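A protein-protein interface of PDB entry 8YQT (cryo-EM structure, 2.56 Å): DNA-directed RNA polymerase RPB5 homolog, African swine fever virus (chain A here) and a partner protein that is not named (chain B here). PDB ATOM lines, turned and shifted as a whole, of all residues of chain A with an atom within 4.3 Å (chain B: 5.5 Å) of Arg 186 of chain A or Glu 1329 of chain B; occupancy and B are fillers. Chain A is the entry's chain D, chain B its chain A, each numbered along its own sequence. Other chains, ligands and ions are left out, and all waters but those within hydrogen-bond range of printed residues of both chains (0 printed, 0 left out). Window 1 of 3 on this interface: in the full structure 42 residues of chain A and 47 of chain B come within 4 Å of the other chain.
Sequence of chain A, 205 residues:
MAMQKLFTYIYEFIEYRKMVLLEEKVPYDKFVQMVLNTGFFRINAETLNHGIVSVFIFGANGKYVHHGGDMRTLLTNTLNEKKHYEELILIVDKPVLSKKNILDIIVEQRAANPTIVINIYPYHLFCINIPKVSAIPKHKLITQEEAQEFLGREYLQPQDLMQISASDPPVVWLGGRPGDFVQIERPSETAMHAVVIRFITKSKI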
ATOM      1  N   PRO A 137      16.022 -21.648 -23.353  1.00  0.00           N
ATOM      2  CA  PRO A 137      15.073 -21.979 -24.426  1.00  0.00           C
ATOM      3  C   PRO A 137      14.289 -23.241 -24.124  1.00  0.00           C
ATOM      4  O   PRO A 137      14.513 -23.871 -23.087  1.00  0.00           O
ATOM      5  CB  PRO A 137      15.978 -22.166 -25.651  1.00  0.00           C
ATOM      6  CG  PRO A 137      17.247 -21.490 -25.305  1.00  0.00           C
ATOM      7  CD  PRO A 137      17.412 -21.644 -23.832  1.00  0.00           C
ATOM      8  N   HIS A 139      13.619 -26.932 -24.286  1.00  0.00           N
ATOM      9  CA  HIS A 139      14.256 -28.202 -24.597  1.00  0.00           C
ATOM     10  C   HIS A 139      13.216 -29.313 -24.592  1.00  0.00           C
ATOM     11  O   HIS A 139      12.261 -29.287 -23.814  1.00  0.00           O
ATOM     12  CB  HIS A 139      15.350 -28.522 -23.579  1.00  0.00           C
ATOM     13  CG  HIS A 139      16.514 -27.583 -23.612  1.00  0.00           C
ATOM     14  ND1 HIS A 139      16.408 -26.253 -23.270  1.00  0.00           N
ATOM     15  CD2 HIS A 139      17.818 -27.793 -23.905  1.00  0.00           C
ATOM     16  CE1 HIS A 139      17.592 -25.678 -23.376  1.00  0.00           C
ATOM     17  NE2 HIS A 139      18.465 -26.591 -23.758  1.00  0.00           N
ATOM     18  N   ILE A 184      15.778 -28.293 -29.424  1.00  0.00           N
ATOM     19  CA  ILE A 184      15.714 -27.028 -28.707  1.00  0.00           C
ATOM     20  C   ILE A 184      15.070 -26.001 -29.622  1.00  0.00           C
ATOM     21  O   ILE A 184      15.591 -25.705 -30.707  1.00  0.00           O
ATOM     22  CB  ILE A 184      17.104 -26.569 -28.250  1.00  0.00           C
ATOM     23  CG1 ILE A 184      17.770 -27.669 -27.424  1.00  0.00           C
ATOM     24  CG2 ILE A 184      17.001 -25.278 -27.465  1.00  0.00           C
ATOM     25  CD1 ILE A 184      19.259 -27.540 -27.331  1.00  0.00           C
ATOM     26  N   GLU A 185      13.931 -25.473 -29.188  1.00  0.00           N
ATOM     27  CA  GLU A 185      13.301 -24.336 -29.839  1.00  0.00           C
ATOM     28  C   GLU A 185      13.735 -23.076 -29.104  1.00  0.00           C
ATOM     29  O   GLU A 185      13.463 -22.924 -27.905  1.00  0.00           O
ATOM     30  CB  GLU A 185      11.782 -24.477 -29.841  1.00  0.00           C
ATOM     31  CG  GLU A 185      11.088 -23.472 -30.735  1.00  0.00           C
ATOM     32  CD  GLU A 185       9.741 -23.959 -31.223  1.00  0.00           C
ATOM     33  OE1 GLU A 185       9.405 -25.134 -30.965  1.00  0.00           O
ATOM     34  OE2 GLU A 185       9.020 -23.167 -31.863  1.00  0.00           O
ATOM     35  N   ARG A 186      14.425 -22.193 -29.814  1.00  0.00           N
ATOM     36  CA  ARG A 186      15.064 -21.053 -29.186  1.00  0.00           C
ATOM     37  C   ARG A 186      14.706 -19.765 -29.908  1.00  0.00           C
ATOM     38  O   ARG A 186      14.493 -19.764 -31.122  1.00  0.00           O
ATOM     39  CB  ARG A 186      16.590 -21.232 -29.156  1.00  0.00           C
ATOM     40  CG  ARG A 186      17.268 -21.378 -30.505  1.00  0.00           C
ATOM     41  CD  ARG A 186      18.684 -21.886 -30.295  1.00  0.00           C
ATOM     42  NE  ARG A 186      19.489 -21.882 -31.509  1.00  0.00           N
ATOM     43  CZ  ARG A 186      20.708 -22.398 -31.597  1.00  0.00           C
ATOM     44  NH1 ARG A 186      21.285 -22.992 -30.566  1.00  0.00           N
ATOM     45  NH2 ARG A 186      21.366 -22.314 -32.749  1.00  0.00           N
ATOM     46  N   PRO A 187      14.615 -18.655 -29.176  1.00  0.00           N
ATOM     47  CA  PRO A 187      14.297 -17.375 -29.816  1.00  0.00           C
ATOM     48  C   PRO A 187      15.419 -16.918 -30.733  1.00  0.00           C
ATOM     49  O   PRO A 187      16.598 -17.182 -30.486  1.00  0.00           O
ATOM     50  CB  PRO A 187      14.122 -16.418 -28.631  1.00  0.00           C
ATOM     51  CG  PRO A 187      13.932 -17.295 -27.447  1.00  0.00           C
ATOM     52  CD  PRO A 187      14.729 -18.520 -27.717  1.00  0.00           C
ATOM     53  N   SER A 188      15.040 -16.223 -31.796  1.00  0.00           N
ATOM     54  CA  SER A 188      15.991 -15.685 -32.753  1.00  0.00           C
ATOM     55  C   SER A 188      15.631 -14.238 -33.041  1.00  0.00           C
ATOM     56  O   SER A 188      14.456 -13.906 -33.205  1.00  0.00           O
ATOM     57  CB  SER A 188      15.994 -16.500 -34.052  1.00  0.00           C
ATOM     58  OG  SER A 188      17.038 -16.090 -34.915  1.00  0.00           O
ATOM     59  N   HIS A 193      12.384 -17.137 -34.429  1.00  0.00           N
ATOM     60  CA  HIS A 193      12.636 -18.353 -33.659  1.00  0.00           C
ATOM     61  C   HIS A 193      13.292 -19.410 -34.537  1.00  0.00           C
ATOM     62  O   HIS A 193      13.119 -19.407 -35.759  1.00  0.00           O
ATOM     63  CB  HIS A 193      11.364 -18.915 -33.009  1.00  0.00           C
ATOM     64  CG  HIS A 193      10.239 -19.171 -33.958  1.00  0.00           C
ATOM     65  ND1 HIS A 193       9.616 -18.169 -34.665  1.00  0.00           N
ATOM     66  CD2 HIS A 193       9.590 -20.314 -34.276  1.00  0.00           C
ATOM     67  CE1 HIS A 193       8.649 -18.686 -35.399  1.00  0.00           C
ATOM     68  NE2 HIS A 193       8.612 -19.987 -35.182  1.00  0.00           N
ATOM     69  N   ALA A 194      14.040 -20.321 -33.921  1.00  0.00           N
ATOM     70  CA  ALA A 194      14.779 -21.345 -34.640  1.00  0.00           C
ATOM     71  C   ALA A 194      14.692 -22.660 -33.882  1.00  0.00           C
ATOM     72  O   ALA A 194      14.375 -22.696 -32.692  1.00  0.00           O
ATOM     73  CB  ALA A 194      16.243 -20.950 -34.839  1.00  0.00           C
ATOM     74  N   VAL A 196      16.958 -26.265 -33.272  1.00  0.00           N
ATOM     75  CA  VAL A 196      18.167 -27.057 -33.440  1.00  0.00           C
ATOM     76  C   VAL A 196      17.956 -28.404 -32.769  1.00  0.00           C
ATOM     77  O   VAL A 196      17.031 -28.597 -31.982  1.00  0.00           O
ATOM     78  CB  VAL A 196      19.422 -26.362 -32.879  1.00  0.00           C
ATOM     79  CG1 VAL A 196      19.731 -25.111 -33.672  1.00  0.00           C
ATOM     80  CG2 VAL A 196      19.244 -26.047 -31.408  1.00  0.00           C
ATOM     81  N   ARG A 198      20.344 -31.288 -30.729  1.00  0.00           N
ATOM     82  CA  ARG A 198      21.631 -31.536 -30.105  1.00  0.00           C
ATOM     83  C   ARG A 198      21.727 -32.983 -29.641  1.00  0.00           C
ATOM     84  O   ARG A 198      20.727 -33.610 -29.280  1.00  0.00           O
ATOM     85  CB  ARG A 198      21.863 -30.592 -28.924  1.00  0.00           C
ATOM     86  CG  ARG A 198      22.345 -29.215 -29.327  1.00  0.00           C
ATOM     87  CD  ARG A 198      22.739 -28.398 -28.122  1.00  0.00           C
ATOM     88  NE  ARG A 198      23.292 -27.105 -28.498  1.00  0.00           N
ATOM     89  CZ  ARG A 198      24.580 -26.799 -28.466  1.00  0.00           C
ATOM     90  NH1 ARG A 198      25.486 -27.669 -28.063  1.00  0.00           N
ATOM     91  NH2 ARG A 198      24.968 -25.586 -28.844  1.00  0.00           N
ATOM     92  N   GLN B 852      25.853 -24.400 -37.148  1.00  0.00           N
ATOM     93  CA  GLN B 852      24.508 -23.856 -37.222  1.00  0.00           C
ATOM     94  C   GLN B 852      23.661 -24.761 -38.098  1.00  0.00           C
ATOM     95  O   GLN B 852      24.125 -25.247 -39.132  1.00  0.00           O
ATOM     96  CB  GLN B 852      24.505 -22.434 -37.790  1.00  0.00           C
ATOM     97  CG  GLN B 852      24.882 -21.374 -36.788  1.00  0.00           C
ATOM     98  CD  GLN B 852      25.101 -20.027 -37.426  1.00  0.00           C
ATOM     99  OE1 GLN B 852      25.321 -19.926 -38.627  1.00  0.00           O
ATOM    100  NE2 GLN B 852      25.033 -18.977 -36.623  1.00  0.00           N
ATOM    101  N   GLU B 857      20.207 -18.484 -38.774  1.00  0.00           N
ATOM    102  CA  GLU B 857      18.892 -19.013 -38.428  1.00  0.00           C
ATOM    103  C   GLU B 857      17.811 -18.577 -39.404  1.00  0.00           C
ATOM    104  O   GLU B 857      16.656 -18.974 -39.239  1.00  0.00           O
ATOM    105  CB  GLU B 857      18.479 -18.648 -36.997  1.00  0.00           C
ATOM    106  CG  GLU B 857      19.282 -19.389 -35.951  1.00  0.00           C
ATOM    107  CD  GLU B 857      19.355 -18.658 -34.635  1.00  0.00           C
ATOM    108  OE1 GLU B 857      18.959 -17.479 -34.587  1.00  0.00           O
ATOM    109  OE2 GLU B 857      19.817 -19.263 -33.647  1.00  0.00           O
ATOM    110  N   GLY B1327      22.975 -23.197 -18.342  1.00  0.00           N
ATOM    111  CA  GLY B1327      23.266 -24.193 -19.348  1.00  0.00           C
ATOM    112  C   GLY B1327      23.962 -23.585 -20.540  1.00  0.00           C
ATOM    113  O   GLY B1327      24.340 -22.411 -20.543  1.00  0.00           O
ATOM    114  N   ILE B1328      24.131 -24.401 -21.579  1.00  0.00           N
ATOM    115  CA  ILE B1328      24.852 -23.959 -22.768  1.00  0.00           C
ATOM    116  C   ILE B1328      23.976 -23.120 -23.694  1.00  0.00           C
ATOM    117  O   ILE B1328      24.483 -22.228 -24.379  1.00  0.00           O
ATOM    118  CB  ILE B1328      25.452 -25.170 -23.511  1.00  0.00           C
ATOM    119  CG1 ILE B1328      26.491 -24.711 -24.532  1.00  0.00           C
ATOM    120  CG2 ILE B1328      24.374 -25.997 -24.189  1.00  0.00           C
ATOM    121  CD1 ILE B1328      27.668 -24.004 -23.925  1.00  0.00           C
ATOM    122  N   GLU B1329      22.668 -23.377 -23.730  1.00  0.00           N
ATOM    123  CA  GLU B1329      21.796 -22.590 -24.590  1.00  0.00           C
ATOM    124  C   GLU B1329      21.585 -21.189 -24.039  1.00  0.00           C
ATOM    125  O   GLU B1329      21.502 -20.224 -24.805  1.00  0.00           O
ATOM    126  CB  GLU B1329      20.464 -23.306 -24.778  1.00  0.00           C
ATOM    127  CG  GLU B1329      20.550 -24.496 -25.704  1.00  0.00           C
ATOM    128  CD  GLU B1329      20.826 -24.092 -27.137  1.00  0.00           C
ATOM    129  OE1 GLU B1329      20.325 -23.032 -27.565  1.00  0.00           O
ATOM    130  OE2 GLU B1329      21.552 -24.829 -27.833  1.00  0.00           O
ATOM    131  N   ALA B1330      21.495 -21.057 -22.715  1.00  0.00           N
ATOM    132  CA  ALA B1330      21.456 -19.732 -22.112  1.00  0.00           C
ATOM    133  C   ALA B1330      22.802 -19.034 -22.216  1.00  0.00           C
ATOM    134  O   ALA B1330      22.852 -17.813 -22.396  1.00  0.00           O
ATOM    135  CB  ALA B1330      21.020 -19.829 -20.656  1.00  0.00           C
ATOM    136  N   ALA B1331      23.899 -19.783 -22.096  1.00  0.00           N
ATOM    137  CA  ALA B1331      25.219 -19.193 -22.277  1.00  0.00           C
ATOM    138  C   ALA B1331      25.443 -18.754 -23.716  1.00  0.00           C
ATOM    139  O   ALA B1331      26.204 -17.814 -23.961  1.00  0.00           O
ATOM    140  CB  ALA B1331      26.301 -20.179 -21.846  1.00  0.00           C
ATOM    141  N   ARG B1332      24.809 -19.426 -24.677  1.00  0.00           N
ATOM    142  CA  ARG B1332      24.871 -18.971 -26.061  1.00  0.00           C
ATOM    143  C   ARG B1332      24.192 -17.619 -26.219  1.00  0.00           C
ATOM    144  O   ARG B1332      24.717 -16.723 -26.888  1.00  0.00           O
ATOM    145  CB  ARG B1332      24.230 -20.007 -26.982  1.00  0.00           C
ATOM    146  CG  ARG B1332      24.578 -19.825 -28.447  1.00  0.00           C
ATOM    147  CD  ARG B1332      23.635 -20.607 -29.331  1.00  0.00           C
ATOM    148  NE  ARG B1332      22.325 -19.978 -29.412  1.00  0.00           N
ATOM    149  CZ  ARG B1332      21.942 -19.166 -30.387  1.00  0.00           C
ATOM    150  NH1 ARG B1332      22.743 -18.878 -31.399  1.00  0.00           N
ATOM    151  NH2 ARG B1332      20.724 -18.636 -30.349  1.00  0.00           N
ATOM    152  N   GLN B1333      23.018 -17.453 -25.605  1.00  0.00           N
ATOM    153  CA  GLN B1333      22.348 -16.159 -25.623  1.00  0.00           C
ATOM    154  C   GLN B1333      23.125 -15.116 -24.834  1.00  0.00           C
ATOM    155  O   GLN B1333      22.988 -13.917 -25.092  1.00  0.00           O
ATOM    156  CB  GLN B1333      20.934 -16.290 -25.059  1.00  0.00           C
ATOM    157  CG  GLN B1333      19.942 -16.989 -25.966  1.00  0.00           C
ATOM    158  CD  GLN B1333      19.694 -16.243 -27.259  1.00  0.00           C
ATOM    159  OE1 GLN B1333      19.943 -15.045 -27.360  1.00  0.00           O
ATOM    160  NE2 GLN B1333      19.186 -16.950 -28.255  1.00  0.00           N
ATOM    161  N   LYS B1334      23.935 -15.546 -23.866  1.00  0.00           N
ATOM    162  CA  LYS B1334      24.720 -14.602 -23.081  1.00  0.00           C
ATOM    163  C   LYS B1334      25.924 -14.087 -23.855  1.00  0.00           C
ATOM    164  O   LYS B1334      26.292 -12.916 -23.724  1.00  0.00           O
ATOM    165  CB  LYS B1334      25.166 -15.249 -21.770  1.00  0.00           C
ATOM    166  CG  LYS B1334      25.812 -14.285 -20.783  1.00  0.00           C
ATOM    167  CD  LYS B1334      24.933 -13.081 -20.518  1.00  0.00           C
ATOM    168  CE  LYS B1334      23.576 -13.488 -19.980  1.00  0.00           C
ATOM    169  NZ  LYS B1334      22.698 -12.308 -19.793  1.00  0.00           N
ATOM    170  N   ASP B1358      27.554 -19.563 -31.665  1.00  0.00           N
ATOM    171  CA  ASP B1358      27.331 -20.936 -32.099  1.00  0.00           C
ATOM    172  C   ASP B1358      28.631 -21.714 -32.208  1.00  0.00           C
ATOM    173  O   ASP B1358      28.660 -22.914 -31.916  1.00  0.00           O
ATOM    174  CB  ASP B1358      26.589 -20.943 -33.430  1.00  0.00           C
ATOM    175  CG  ASP B1358      25.094 -20.863 -33.254  1.00  0.00           C
ATOM    176  OD1 ASP B1358      24.545 -21.671 -32.481  1.00  0.00           O
ATOM    177  OD2 ASP B1358      24.466 -19.979 -33.870  1.00  0.00           O
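OE2 of Glu 857 of chain B lies within salt-bridge range of NE of Arg 186 of chain A, at 3.4 Å.
The backbone carbonyl oxygen of Pro 187 of chain A is in hydrogen-bond range of the side-chain amide nitrogen of Gln 1333 of chain B, 3.4 Å away.
The side-chain carboxylate of Glu 857 of chain B lies close to the side-chain hydroxyl of Ser 188 of chain A.
The side-chain carboxylate (OE2) of Glu 1329 of chain B is in salt-bridge range of the guanidinium group (NE) of Arg 198 of chain A (2.9 Å).
The guanidinium group (NE) of Arg 1332 of chain B lies close to the guanidinium group (NH1) of Arg 186 of chain A, at 3.4 Å.
OE1 of Glu 1329 of chain B is in salt-bridge range of NH1 of Arg 186 of chain A (3.2 Å).
The side-chain carboxylate (OD1) of Asp 1358 of chain B lies within salt-bridge range of the guanidinium group (NH2) of Arg 186 of chain A, at 3.3 Å.
The backbone carbonyl oxygen (O) of Arg 186 of chain A is in hydrogen-bond range of the backbone NH (N) of Ala 194 of chain A (2.9 Å).
The side-chain carboxylate (OD2) of Asp 1358 of chain B is in salt-bridge range of the guanidinium group (NH1) of Arg 1332 of chain B (3.2 Å).
NE2 of Gln 852 of chain B sits at hydrogen-bond distance from OD2 of Asp 1358 of chain B.
The backbone NH (N) of Ile 184 of chain A lies within hydrogen-bond range of the backbone carbonyl oxygen (O) of Val 196 of chain A (2.9 Å).
The side-chain carboxylate of Glu 857 of chain B is in salt-bridge range of the guanidinium group of Arg 1332 of chain B (3.5 Å).
The backbone carbonyl oxygen (O) of Pro 137 of chain A lies within hydrogen-bond range of a ring nitrogen (ND1) of His 139 of chain A (3.0 Å).
Among the printed residues, pairs that only touch across the chains: Pro 137 of chain A with Glu 1329 of chain B (3.6 Å), His 139 of chain A with Glu 1329 of chain B (3.5 Å), Ile 184 of chain A with Glu 1329 of chain B (3.6 Å) and Ala 194 of chain A with Glu 857 of chain B (3.6 Å).
Of the printed residues of chain B, Ile 184 of chain A touches Glu 1329.
Printed residues of chain B within 4 Å of Pro 187 of chain A: Gln 1333.
Printed residues of chain B within 4 Å of Ser 188 of chain A: Glu 857 (2.4 Å).
Of chain A, only Pro 137 (3.6 Å), His 139 (3.5 Å), Ile 184 (3.6 Å), Arg 186 (3.2 Å) and Arg 198 (2.9 Å) come within 4 Å of Glu 1329 of chain B.
The nearest printed residue of chain A that does not touch Glu 1329 of chain B is Val 196 of chain A (4.4 Å).
The nearest printed residue of chain B that does not touch His 139 of chain A is Ile 1328 of chain B (6.0 Å).
Along chain B the printed residues that touch a printed residue of chain A span positions 857 to 1358.
Printed residues of chain A that touch a printed residue of chain B: Pro 137, His 139, Ile 184, Arg 186, Pro 187, Ser 188, Ala 194 and Arg 198.
Hydrophobic or aromatic side chains of chain A that line the printed part of chain B: Pro 137, His 139, Ile 184 and Ala 194.
Among the printed residues, 11 pairs touch across the chains.
Among the printed residues, Asp or Glu carboxylates within 4 Å of a Lys or Arg side-chain nitrogen of the other chain: Arg 186 of chain A with Glu 857 of chain B (3.4 Å), Arg 186 of chain A with Glu 1329 of chain B (3.2 Å), Arg 186 of chain A with Asp 1358 of chain B (3.3 Å) and Arg 198 of chain A with Glu 1329 of chain B (2.9 Å).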
